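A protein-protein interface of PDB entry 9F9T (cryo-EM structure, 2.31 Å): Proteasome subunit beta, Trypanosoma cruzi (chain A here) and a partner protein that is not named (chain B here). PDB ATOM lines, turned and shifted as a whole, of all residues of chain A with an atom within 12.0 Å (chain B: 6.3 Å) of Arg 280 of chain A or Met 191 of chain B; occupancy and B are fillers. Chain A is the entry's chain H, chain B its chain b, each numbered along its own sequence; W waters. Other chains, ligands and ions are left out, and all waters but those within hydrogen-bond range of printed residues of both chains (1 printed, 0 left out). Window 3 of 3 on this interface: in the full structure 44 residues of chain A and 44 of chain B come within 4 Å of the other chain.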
ATOM      1  N   LEU A 261       6.813 -25.640  20.491  1.00  0.00           N
ATOM      2  CA  LEU A 261       5.752 -24.662  20.335  1.00  0.00           C
ATOM      3  C   LEU A 261       4.448 -25.218  20.878  1.00  0.00           C
ATOM      4  O   LEU A 261       4.164 -26.393  20.718  1.00  0.00           O
ATOM      5  CB  LEU A 261       5.557 -24.287  18.862  1.00  0.00           C
ATOM      6  CG  LEU A 261       6.670 -23.491  18.190  1.00  0.00           C
ATOM      7  CD1 LEU A 261       6.403 -23.304  16.714  1.00  0.00           C
ATOM      8  CD2 LEU A 261       6.889 -22.143  18.839  1.00  0.00           C
ATOM      9  N   ASN A 265      -2.453 -25.303  16.630  1.00  0.00           N
ATOM     10  CA  ASN A 265      -2.852 -25.446  15.245  1.00  0.00           C
ATOM     11  C   ASN A 265      -2.815 -26.905  14.847  1.00  0.00           C
ATOM     12  O   ASN A 265      -2.155 -27.293  13.902  1.00  0.00           O
ATOM     13  CB  ASN A 265      -1.996 -24.591  14.314  1.00  0.00           C
ATOM     14  CG  ASN A 265      -2.035 -23.084  14.543  1.00  0.00           C
ATOM     15  OD1 ASN A 265      -2.975 -22.508  15.081  1.00  0.00           O
ATOM     16  ND2 ASN A 265      -0.935 -22.424  14.255  1.00  0.00           N
ATOM     17  N   PRO A 266      -3.543 -27.789  15.545  1.00  0.00           N
ATOM     18  CA  PRO A 266      -3.564 -29.201  15.182  1.00  0.00           C
ATOM     19  C   PRO A 266      -4.291 -29.430  13.864  1.00  0.00           C
ATOM     20  O   PRO A 266      -5.209 -28.689  13.520  1.00  0.00           O
ATOM     21  CB  PRO A 266      -4.407 -29.770  16.344  1.00  0.00           C
ATOM     22  CG  PRO A 266      -5.425 -28.667  16.635  1.00  0.00           C
ATOM     23  CD  PRO A 266      -4.509 -27.467  16.613  1.00  0.00           C
ATOM     24  N   PRO A 267      -3.912 -30.476  13.107  1.00  0.00           N
ATOM     25  CA  PRO A 267      -4.572 -30.797  11.853  1.00  0.00           C
ATOM     26  C   PRO A 267      -5.972 -31.323  12.070  1.00  0.00           C
ATOM     27  O   PRO A 267      -6.250 -32.008  13.059  1.00  0.00           O
ATOM     28  CB  PRO A 267      -3.885 -32.044  11.282  1.00  0.00           C
ATOM     29  CG  PRO A 267      -2.821 -32.447  12.280  1.00  0.00           C
ATOM     30  CD  PRO A 267      -2.826 -31.421  13.407  1.00  0.00           C
ATOM     31  N   PHE A 268      -6.794 -31.090  11.072  1.00  0.00           N
ATOM     32  CA  PHE A 268      -8.103 -31.689  10.959  1.00  0.00           C
ATOM     33  C   PHE A 268      -7.979 -33.211  11.024  1.00  0.00           C
ATOM     34  O   PHE A 268      -7.339 -33.820  10.166  1.00  0.00           O
ATOM     35  CB  PHE A 268      -8.736 -31.148   9.672  1.00  0.00           C
ATOM     36  CG  PHE A 268     -10.174 -31.496   9.473  1.00  0.00           C
ATOM     37  CD1 PHE A 268     -11.088 -31.309  10.492  1.00  0.00           C
ATOM     38  CD2 PHE A 268     -10.635 -31.915   8.230  1.00  0.00           C
ATOM     39  CE1 PHE A 268     -12.426 -31.616  10.308  1.00  0.00           C
ATOM     40  CE2 PHE A 268     -11.984 -32.218   8.049  1.00  0.00           C
ATOM     41  CZ  PHE A 268     -12.861 -32.089   9.097  1.00  0.00           C
ATOM     42  N   SER A 269      -8.599 -33.810  12.044  1.00  0.00           N
ATOM     43  CA  SER A 269      -8.378 -35.208  12.372  1.00  0.00           C
ATOM     44  C   SER A 269      -9.663 -35.898  12.764  1.00  0.00           C
ATOM     45  O   SER A 269     -10.662 -35.263  13.090  1.00  0.00           O
ATOM     46  CB  SER A 269      -7.392 -35.368  13.506  1.00  0.00           C
ATOM     47  OG  SER A 269      -8.004 -34.939  14.698  1.00  0.00           O
ATOM     48  N   VAL A 276       0.638 -32.636  17.538  1.00  0.00           N
ATOM     49  CA  VAL A 276       1.558 -31.684  16.947  1.00  0.00           C
ATOM     50  C   VAL A 276       0.783 -30.618  16.169  1.00  0.00           C
ATOM     51  O   VAL A 276      -0.377 -30.798  15.830  1.00  0.00           O
ATOM     52  CB  VAL A 276       2.571 -32.401  16.042  1.00  0.00           C
ATOM     53  CG1 VAL A 276       3.366 -33.397  16.848  1.00  0.00           C
ATOM     54  CG2 VAL A 276       1.908 -33.076  14.858  1.00  0.00           C
ATOM     55  N   ASN A 277       1.442 -29.477  15.974  1.00  0.00           N
ATOM     56  CA  ASN A 277       0.978 -28.458  15.064  1.00  0.00           C
ATOM     57  C   ASN A 277       1.088 -28.978  13.627  1.00  0.00           C
ATOM     58  O   ASN A 277       2.040 -29.673  13.268  1.00  0.00           O
ATOM     59  CB  ASN A 277       1.781 -27.184  15.279  1.00  0.00           C
ATOM     60  CG  ASN A 277       1.387 -26.408  16.519  1.00  0.00           C
ATOM     61  OD1 ASN A 277       0.237 -25.977  16.627  1.00  0.00           O
ATOM     62  ND2 ASN A 277       2.338 -26.117  17.402  1.00  0.00           N
ATOM     63  N   GLN A 278       0.069 -28.682  12.817  1.00  0.00           N
ATOM     64  CA  GLN A 278       0.144 -28.911  11.377  1.00  0.00           C
ATOM     65  C   GLN A 278       1.232 -28.012  10.757  1.00  0.00           C
ATOM     66  O   GLN A 278       1.227 -26.800  11.003  1.00  0.00           O
ATOM     67  CB  GLN A 278      -1.193 -28.592  10.747  1.00  0.00           C
ATOM     68  CG  GLN A 278      -1.299 -29.073   9.332  1.00  0.00           C
ATOM     69  CD  GLN A 278      -2.526 -28.603   8.584  1.00  0.00           C
ATOM     70  OE1 GLN A 278      -3.570 -28.262   9.132  1.00  0.00           O
ATOM     71  NE2 GLN A 278      -2.434 -28.695   7.277  1.00  0.00           N
ATOM     72  N   SER A 279       2.169 -28.613  10.016  1.00  0.00           N
ATOM     73  CA  SER A 279       3.318 -27.918   9.432  1.00  0.00           C
ATOM     74  C   SER A 279       3.223 -27.794   7.901  1.00  0.00           C
ATOM     75  O   SER A 279       3.844 -26.906   7.355  1.00  0.00           O
ATOM     76  CB  SER A 279       4.582 -28.622   9.791  1.00  0.00           C
ATOM     77  OG  SER A 279       4.584 -29.961   9.295  1.00  0.00           O
ATOM     78  N   ARG A 280       2.441 -28.647   7.225  1.00  0.00           N
ATOM     79  CA  ARG A 280       2.334 -28.659   5.783  1.00  0.00           C
ATOM     80  C   ARG A 280       0.875 -28.844   5.355  1.00  0.00           C
ATOM     81  O   ARG A 280       0.100 -29.525   5.999  1.00  0.00           O
ATOM     82  CB  ARG A 280       3.266 -29.725   5.212  1.00  0.00           C
ATOM     83  CG  ARG A 280       2.800 -31.147   5.470  1.00  0.00           C
ATOM     84  CD  ARG A 280       3.766 -32.211   4.947  1.00  0.00           C
ATOM     85  NE  ARG A 280       5.084 -31.671   4.616  1.00  0.00           N
ATOM     86  CZ  ARG A 280       5.563 -31.577   3.378  1.00  0.00           C
ATOM     87  NH1 ARG A 280       6.685 -30.910   3.160  1.00  0.00           N
ATOM     88  NH2 ARG A 280       4.896 -32.105   2.359  1.00  0.00           N
ATOM     89  N   SER A 281       0.487 -28.176   4.297  1.00  0.00           N
ATOM     90  CA  SER A 281      -0.822 -28.370   3.701  1.00  0.00           C
ATOM     91  C   SER A 281      -1.111 -29.843   3.470  1.00  0.00           C
ATOM     92  O   SER A 281      -0.221 -30.626   3.212  1.00  0.00           O
ATOM     93  CB  SER A 281      -0.923 -27.628   2.359  1.00  0.00           C
ATOM     94  OG  SER A 281      -0.766 -26.221   2.494  1.00  0.00           O
ATOM     95  N   GLU A 282      -2.393 -30.188   3.568  1.00  0.00           N
ATOM     96  CA  GLU A 282      -2.911 -31.476   3.148  1.00  0.00           C
ATOM     97  C   GLU A 282      -3.215 -31.457   1.642  1.00  0.00           C
ATOM     98  O   GLU A 282      -2.943 -32.497   0.976  1.00  0.00           O
ATOM     99  CB  GLU A 282      -4.157 -31.765   3.977  1.00  0.00           C
ATOM    100  CG  GLU A 282      -3.869 -32.552   5.247  1.00  0.00           C
ATOM    101  CD  GLU A 282      -3.747 -34.066   5.068  1.00  0.00           C
ATOM    102  OE1 GLU A 282      -4.754 -34.783   5.323  1.00  0.00           O
ATOM    103  OE2 GLU A 282      -2.639 -34.543   4.707  1.00  0.00           O
ATOM    104  N   LEU B  40      -2.611 -22.845   8.539  1.00  0.00           N
ATOM    105  CA  LEU B  40      -2.876 -23.400   7.237  1.00  0.00           C
ATOM    106  C   LEU B  40      -4.368 -23.507   6.998  1.00  0.00           C
ATOM    107  O   LEU B  40      -5.095 -24.073   7.780  1.00  0.00           O
ATOM    108  CB  LEU B  40      -2.261 -24.775   7.159  1.00  0.00           C
ATOM    109  CG  LEU B  40      -0.739 -24.830   7.311  1.00  0.00           C
ATOM    110  CD1 LEU B  40      -0.254 -26.201   6.948  1.00  0.00           C
ATOM    111  CD2 LEU B  40       0.011 -23.799   6.461  1.00  0.00           C
ATOM    112  N   ALA B  43      -5.792 -26.459   1.208  1.00  0.00           N
ATOM    113  CA  ALA B  43      -4.625 -27.074   0.605  1.00  0.00           C
ATOM    114  C   ALA B  43      -3.522 -26.078   0.224  1.00  0.00           C
ATOM    115  O   ALA B  43      -2.364 -26.447   0.093  1.00  0.00           O
ATOM    116  CB  ALA B  43      -5.078 -27.865  -0.630  1.00  0.00           C
ATOM    117  N   TYR B  44      -3.895 -24.840  -0.092  1.00  0.00           N
ATOM    118  CA  TYR B  44      -2.962 -23.960  -0.768  1.00  0.00           C
ATOM    119  C   TYR B  44      -2.651 -22.719   0.003  1.00  0.00           C
ATOM    120  O   TYR B  44      -2.107 -21.861  -0.617  1.00  0.00           O
ATOM    121  CB  TYR B  44      -3.685 -23.449  -2.038  1.00  0.00           C
ATOM    122  CG  TYR B  44      -4.196 -24.556  -2.910  1.00  0.00           C
ATOM    123  CD1 TYR B  44      -3.299 -25.463  -3.476  1.00  0.00           C
ATOM    124  CD2 TYR B  44      -5.561 -24.839  -2.987  1.00  0.00           C
ATOM    125  CE1 TYR B  44      -3.738 -26.592  -4.164  1.00  0.00           C
ATOM    126  CE2 TYR B  44      -6.029 -25.960  -3.692  1.00  0.00           C
ATOM    127  CZ  TYR B  44      -5.110 -26.830  -4.289  1.00  0.00           C
ATOM    128  OH  TYR B  44      -5.527 -27.889  -5.054  1.00  0.00           O
ATOM    129  N   THR B  45      -3.196 -22.525   1.188  1.00  0.00           N
ATOM    130  CA  THR B  45      -3.288 -21.183   1.693  1.00  0.00           C
ATOM    131  C   THR B  45      -2.841 -21.134   3.140  1.00  0.00           C
ATOM    132  O   THR B  45      -2.997 -22.098   3.860  1.00  0.00           O
ATOM    133  CB  THR B  45      -4.714 -20.630   1.654  1.00  0.00           C
ATOM    134  OG1 THR B  45      -5.305 -20.792   0.365  1.00  0.00           O
ATOM    135  CG2 THR B  45      -4.738 -19.171   2.120  1.00  0.00           C
ATOM    136  N   CYS B 110      -0.446 -20.543  -2.946  1.00  0.00           N
ATOM    137  CA  CYS B 110       0.064 -20.942  -4.241  1.00  0.00           C
ATOM    138  C   CYS B 110      -0.897 -21.934  -4.858  1.00  0.00           C
ATOM    139  O   CYS B 110      -1.130 -22.975  -4.285  1.00  0.00           O
ATOM    140  CB  CYS B 110       1.461 -21.551  -4.115  1.00  0.00           C
ATOM    141  SG  CYS B 110       2.351 -21.695  -5.701  1.00  0.00           S
ATOM    142  N   HIS B 111      -1.465 -21.593  -6.005  1.00  0.00           N
ATOM    143  CA  HIS B 111      -2.318 -22.499  -6.771  1.00  0.00           C
ATOM    144  C   HIS B 111      -2.121 -22.210  -8.266  1.00  0.00           C
ATOM    145  O   HIS B 111      -2.075 -21.064  -8.696  1.00  0.00           O
ATOM    146  CB  HIS B 111      -3.775 -22.304  -6.332  1.00  0.00           C
ATOM    147  CG  HIS B 111      -4.815 -23.035  -7.081  1.00  0.00           C
ATOM    148  ND1 HIS B 111      -5.590 -22.395  -8.030  1.00  0.00           N
ATOM    149  CD2 HIS B 111      -5.152 -24.342  -7.102  1.00  0.00           C
ATOM    150  CE1 HIS B 111      -6.419 -23.299  -8.573  1.00  0.00           C
ATOM    151  NE2 HIS B 111      -6.149 -24.490  -8.052  1.00  0.00           N
ATOM    152  N   ASP B 186       6.407 -21.009   3.411  1.00  0.00           N
ATOM    153  CA  ASP B 186       6.812 -20.923   2.031  1.00  0.00           C
ATOM    154  C   ASP B 186       5.684 -21.609   1.263  1.00  0.00           C
ATOM    155  O   ASP B 186       5.481 -22.834   1.421  1.00  0.00           O
ATOM    156  CB  ASP B 186       8.173 -21.601   1.843  1.00  0.00           C
ATOM    157  CG  ASP B 186       8.844 -21.501   0.466  1.00  0.00           C
ATOM    158  OD1 ASP B 186       8.832 -20.404  -0.180  1.00  0.00           O
ATOM    159  OD2 ASP B 186       9.440 -22.522   0.045  1.00  0.00           O
ATOM    160  N   ALA B 187       4.964 -20.811   0.463  1.00  0.00           N
ATOM    161  CA  ALA B 187       3.995 -21.370  -0.482  1.00  0.00           C
ATOM    162  C   ALA B 187       4.686 -21.567  -1.828  1.00  0.00           C
ATOM    163  O   ALA B 187       5.168 -20.600  -2.396  1.00  0.00           O
ATOM    164  CB  ALA B 187       2.773 -20.429  -0.583  1.00  0.00           C
ATOM    165  N   THR B 188       4.677 -22.784  -2.371  1.00  0.00           N
ATOM    166  CA  THR B 188       5.350 -23.064  -3.626  1.00  0.00           C
ATOM    167  C   THR B 188       4.994 -24.485  -4.038  1.00  0.00           C
ATOM    168  O   THR B 188       4.816 -25.339  -3.190  1.00  0.00           O
ATOM    169  CB  THR B 188       6.869 -22.805  -3.481  1.00  0.00           C
ATOM    170  OG1 THR B 188       7.676 -22.785  -4.664  1.00  0.00           O
ATOM    171  CG2 THR B 188       7.557 -23.824  -2.611  1.00  0.00           C
ATOM    172  N   SER B 189       4.836 -24.703  -5.351  1.00  0.00           N
ATOM    173  CA  SER B 189       4.423 -25.973  -5.922  1.00  0.00           C
ATOM    174  C   SER B 189       3.096 -26.427  -5.338  1.00  0.00           C
ATOM    175  O   SER B 189       2.937 -27.611  -5.023  1.00  0.00           O
ATOM    176  CB  SER B 189       5.494 -27.040  -5.718  1.00  0.00           C
ATOM    177  OG  SER B 189       6.506 -26.936  -6.723  1.00  0.00           O
ATOM    178  N   ASP B 190       2.190 -25.462  -5.158  1.00  0.00           N
ATOM    179  CA  ASP B 190       0.786 -25.743  -4.881  1.00  0.00           C
ATOM    180  C   ASP B 190       0.644 -26.372  -3.484  1.00  0.00           C
ATOM    181  O   ASP B 190      -0.188 -27.246  -3.234  1.00  0.00           O
ATOM    182  CB  ASP B 190       0.158 -26.586  -6.008  1.00  0.00           C
ATOM    183  CG  ASP B 190      -0.328 -25.810  -7.235  1.00  0.00           C
ATOM    184  OD1 ASP B 190       0.519 -25.350  -8.046  1.00  0.00           O
ATOM    185  OD2 ASP B 190      -1.581 -25.719  -7.411  1.00  0.00           O
ATOM    186  N   MET B 191       1.437 -25.876  -2.546  1.00  0.00           N
ATOM    187  CA  MET B 191       1.354 -26.360  -1.189  1.00  0.00           C
ATOM    188  C   MET B 191       2.148 -25.444  -0.274  1.00  0.00           C
ATOM    189  O   MET B 191       3.113 -24.841  -0.708  1.00  0.00           O
ATOM    190  CB  MET B 191       1.904 -27.779  -1.082  1.00  0.00           C
ATOM    191  CG  MET B 191       3.310 -27.948  -1.532  1.00  0.00           C
ATOM    192  SD  MET B 191       3.688 -29.746  -1.375  1.00  0.00           S
ATOM    193  CE  MET B 191       4.264 -29.740   0.334  1.00  0.00           C
ATOM    194  N   VAL B 192       1.762 -25.394   0.995  1.00  0.00           N
ATOM    195  CA  VAL B 192       2.459 -24.551   1.935  1.00  0.00           C
ATOM    196  C   VAL B 192       3.186 -25.426   2.947  1.00  0.00           C
ATOM    197  O   VAL B 192       2.699 -26.499   3.279  1.00  0.00           O
ATOM    198  CB  VAL B 192       1.473 -23.626   2.618  1.00  0.00           C
ATOM    199  CG1 VAL B 192       2.203 -22.590   3.431  1.00  0.00           C
ATOM    200  CG2 VAL B 192       0.571 -22.927   1.626  1.00  0.00           C
ATOM    201  N   SER B 193       4.316 -24.937   3.442  1.00  0.00           N
ATOM    202  CA  SER B 193       5.066 -25.636   4.462  1.00  0.00           C
ATOM    203  C   SER B 193       5.580 -24.618   5.475  1.00  0.00           C
ATOM    204  O   SER B 193       6.150 -23.593   5.099  1.00  0.00           O
ATOM    205  CB  SER B 193       6.260 -26.395   3.868  1.00  0.00           C
ATOM    206  OG  SER B 193       7.466 -25.651   4.026  1.00  0.00           O
ATOM    207  N   ILE B 194       5.504 -24.958   6.762  1.00  0.00           N
ATOM    208  CA  ILE B 194       5.953 -24.043   7.799  1.00  0.00           C
ATOM    209  C   ILE B 194       7.235 -24.561   8.421  1.00  0.00           C
ATOM    210  O   ILE B 194       7.317 -25.742   8.771  1.00  0.00           O
ATOM    211  CB  ILE B 194       4.818 -23.829   8.807  1.00  0.00           C
ATOM    212  CG1 ILE B 194       3.634 -23.146   8.129  1.00  0.00           C
ATOM    213  CG2 ILE B 194       5.305 -22.973   9.933  1.00  0.00           C
ATOM    214  CD1 ILE B 194       2.464 -23.041   9.058  1.00  0.00           C
HETATM  215  O   HOH W   1      -2.648 -24.788   3.341  1.00  0.00           O
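The backbone carbonyl oxygen (O) of Ala 43 of chain B lies within hydrogen-bond range of the side-chain hydroxyl (OG) of Ser 281 of chain A (2.9 Å).
O of Val 192 of chain B sits at hydrogen-bond distance from N of Ser 281 of chain A (3.0 Å).
N of Ile 194 of chain B lies within hydrogen-bond range of O of Ser 279 of chain A (2.6 Å).
N of Gln 278 of chain A is in hydrogen-bond range of O of Asn 265 of chain A.
The backbone NH of Asp 186 of chain B sits at hydrogen-bond distance from the backbone carbonyl oxygen of Ser 193 of chain B (3.1 Å).
O of Arg 280 of chain A sits at hydrogen-bond distance from NE2 of Gln 278 of chain A (3.0 Å).
Among the printed residues, pairs that only touch across the chains: Arg 280 of chain A with Met 191 of chain B (3.2 Å), Arg 280 of chain A with Leu 40 of chain B (3.3 Å), Arg 280 of chain A with Val 192 of chain B (3.3 Å), Gln 278 of chain A with Leu 40 of chain B (3.3 Å), Ser 279 of chain A with Ser 193 of chain B (3.4 Å), Ser 281 of chain A with Leu 40 of chain B (3.4 Å) and Ser 279 of chain A with Leu 40 of chain B (3.9 Å).
Of the printed residues of chain B, Ser 279 of chain A touches Leu 40, Ser 193 and Ile 194.
Arg 280 of chain A touches just these residues of chain B: Leu 40, Met 191 and Val 192.
Printed residues of chain B within 4 Å of Ser 281 of chain A: Leu 40, Ala 43 and Val 192.
Leu 40 of chain B touches just these residues of chain A: Gln 278, Ser 279, Arg 280 and Ser 281.
Of chain A, only Ser 281 comes within 4 Å of Ala 43 of chain B.
No residue of chain A comes within 4 Å of Cys 110 of chain B.
No residue of chain A comes within 4 Å of Asp 186 of chain B.
No residue of chain A comes within 4 Å of Ala 187 of chain B.
No residue of chain A comes within 4 Å of Thr 188 of chain B.
Of chain A, only Arg 280 comes within 4 Å of Met 191 of chain B.
Of chain A, only Arg 280 and Ser 281 come within 4 Å of Val 192 of chain B.
Of the printed residues of chain A, Ser 193 of chain B touches Ser 279 (3.4 Å).
Of chain A, only Ser 279 (2.6 Å) comes within 4 Å of Ile 194 of chain B.
The nearest residue of chain A that does not touch Met 191 of chain B is Ser 281 of chain A (4.1 Å).
Of the 13 printed residues of chain A, 4 touch a printed residue of chain B.
Of the 15 printed residues of chain B, 6 touch a printed residue of chain A.
Hydrophobic or aromatic side chains of chain B that line the printed part of chain A: Leu 40, Met 191, Val 192 and Ile 194.
Among the printed residues, 10 pairs touch across the chains.
Water W1 bridges OG of Ser 281 of chain A (2.5 Å) and O of Thr 45 of chain B (2.8 Å).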
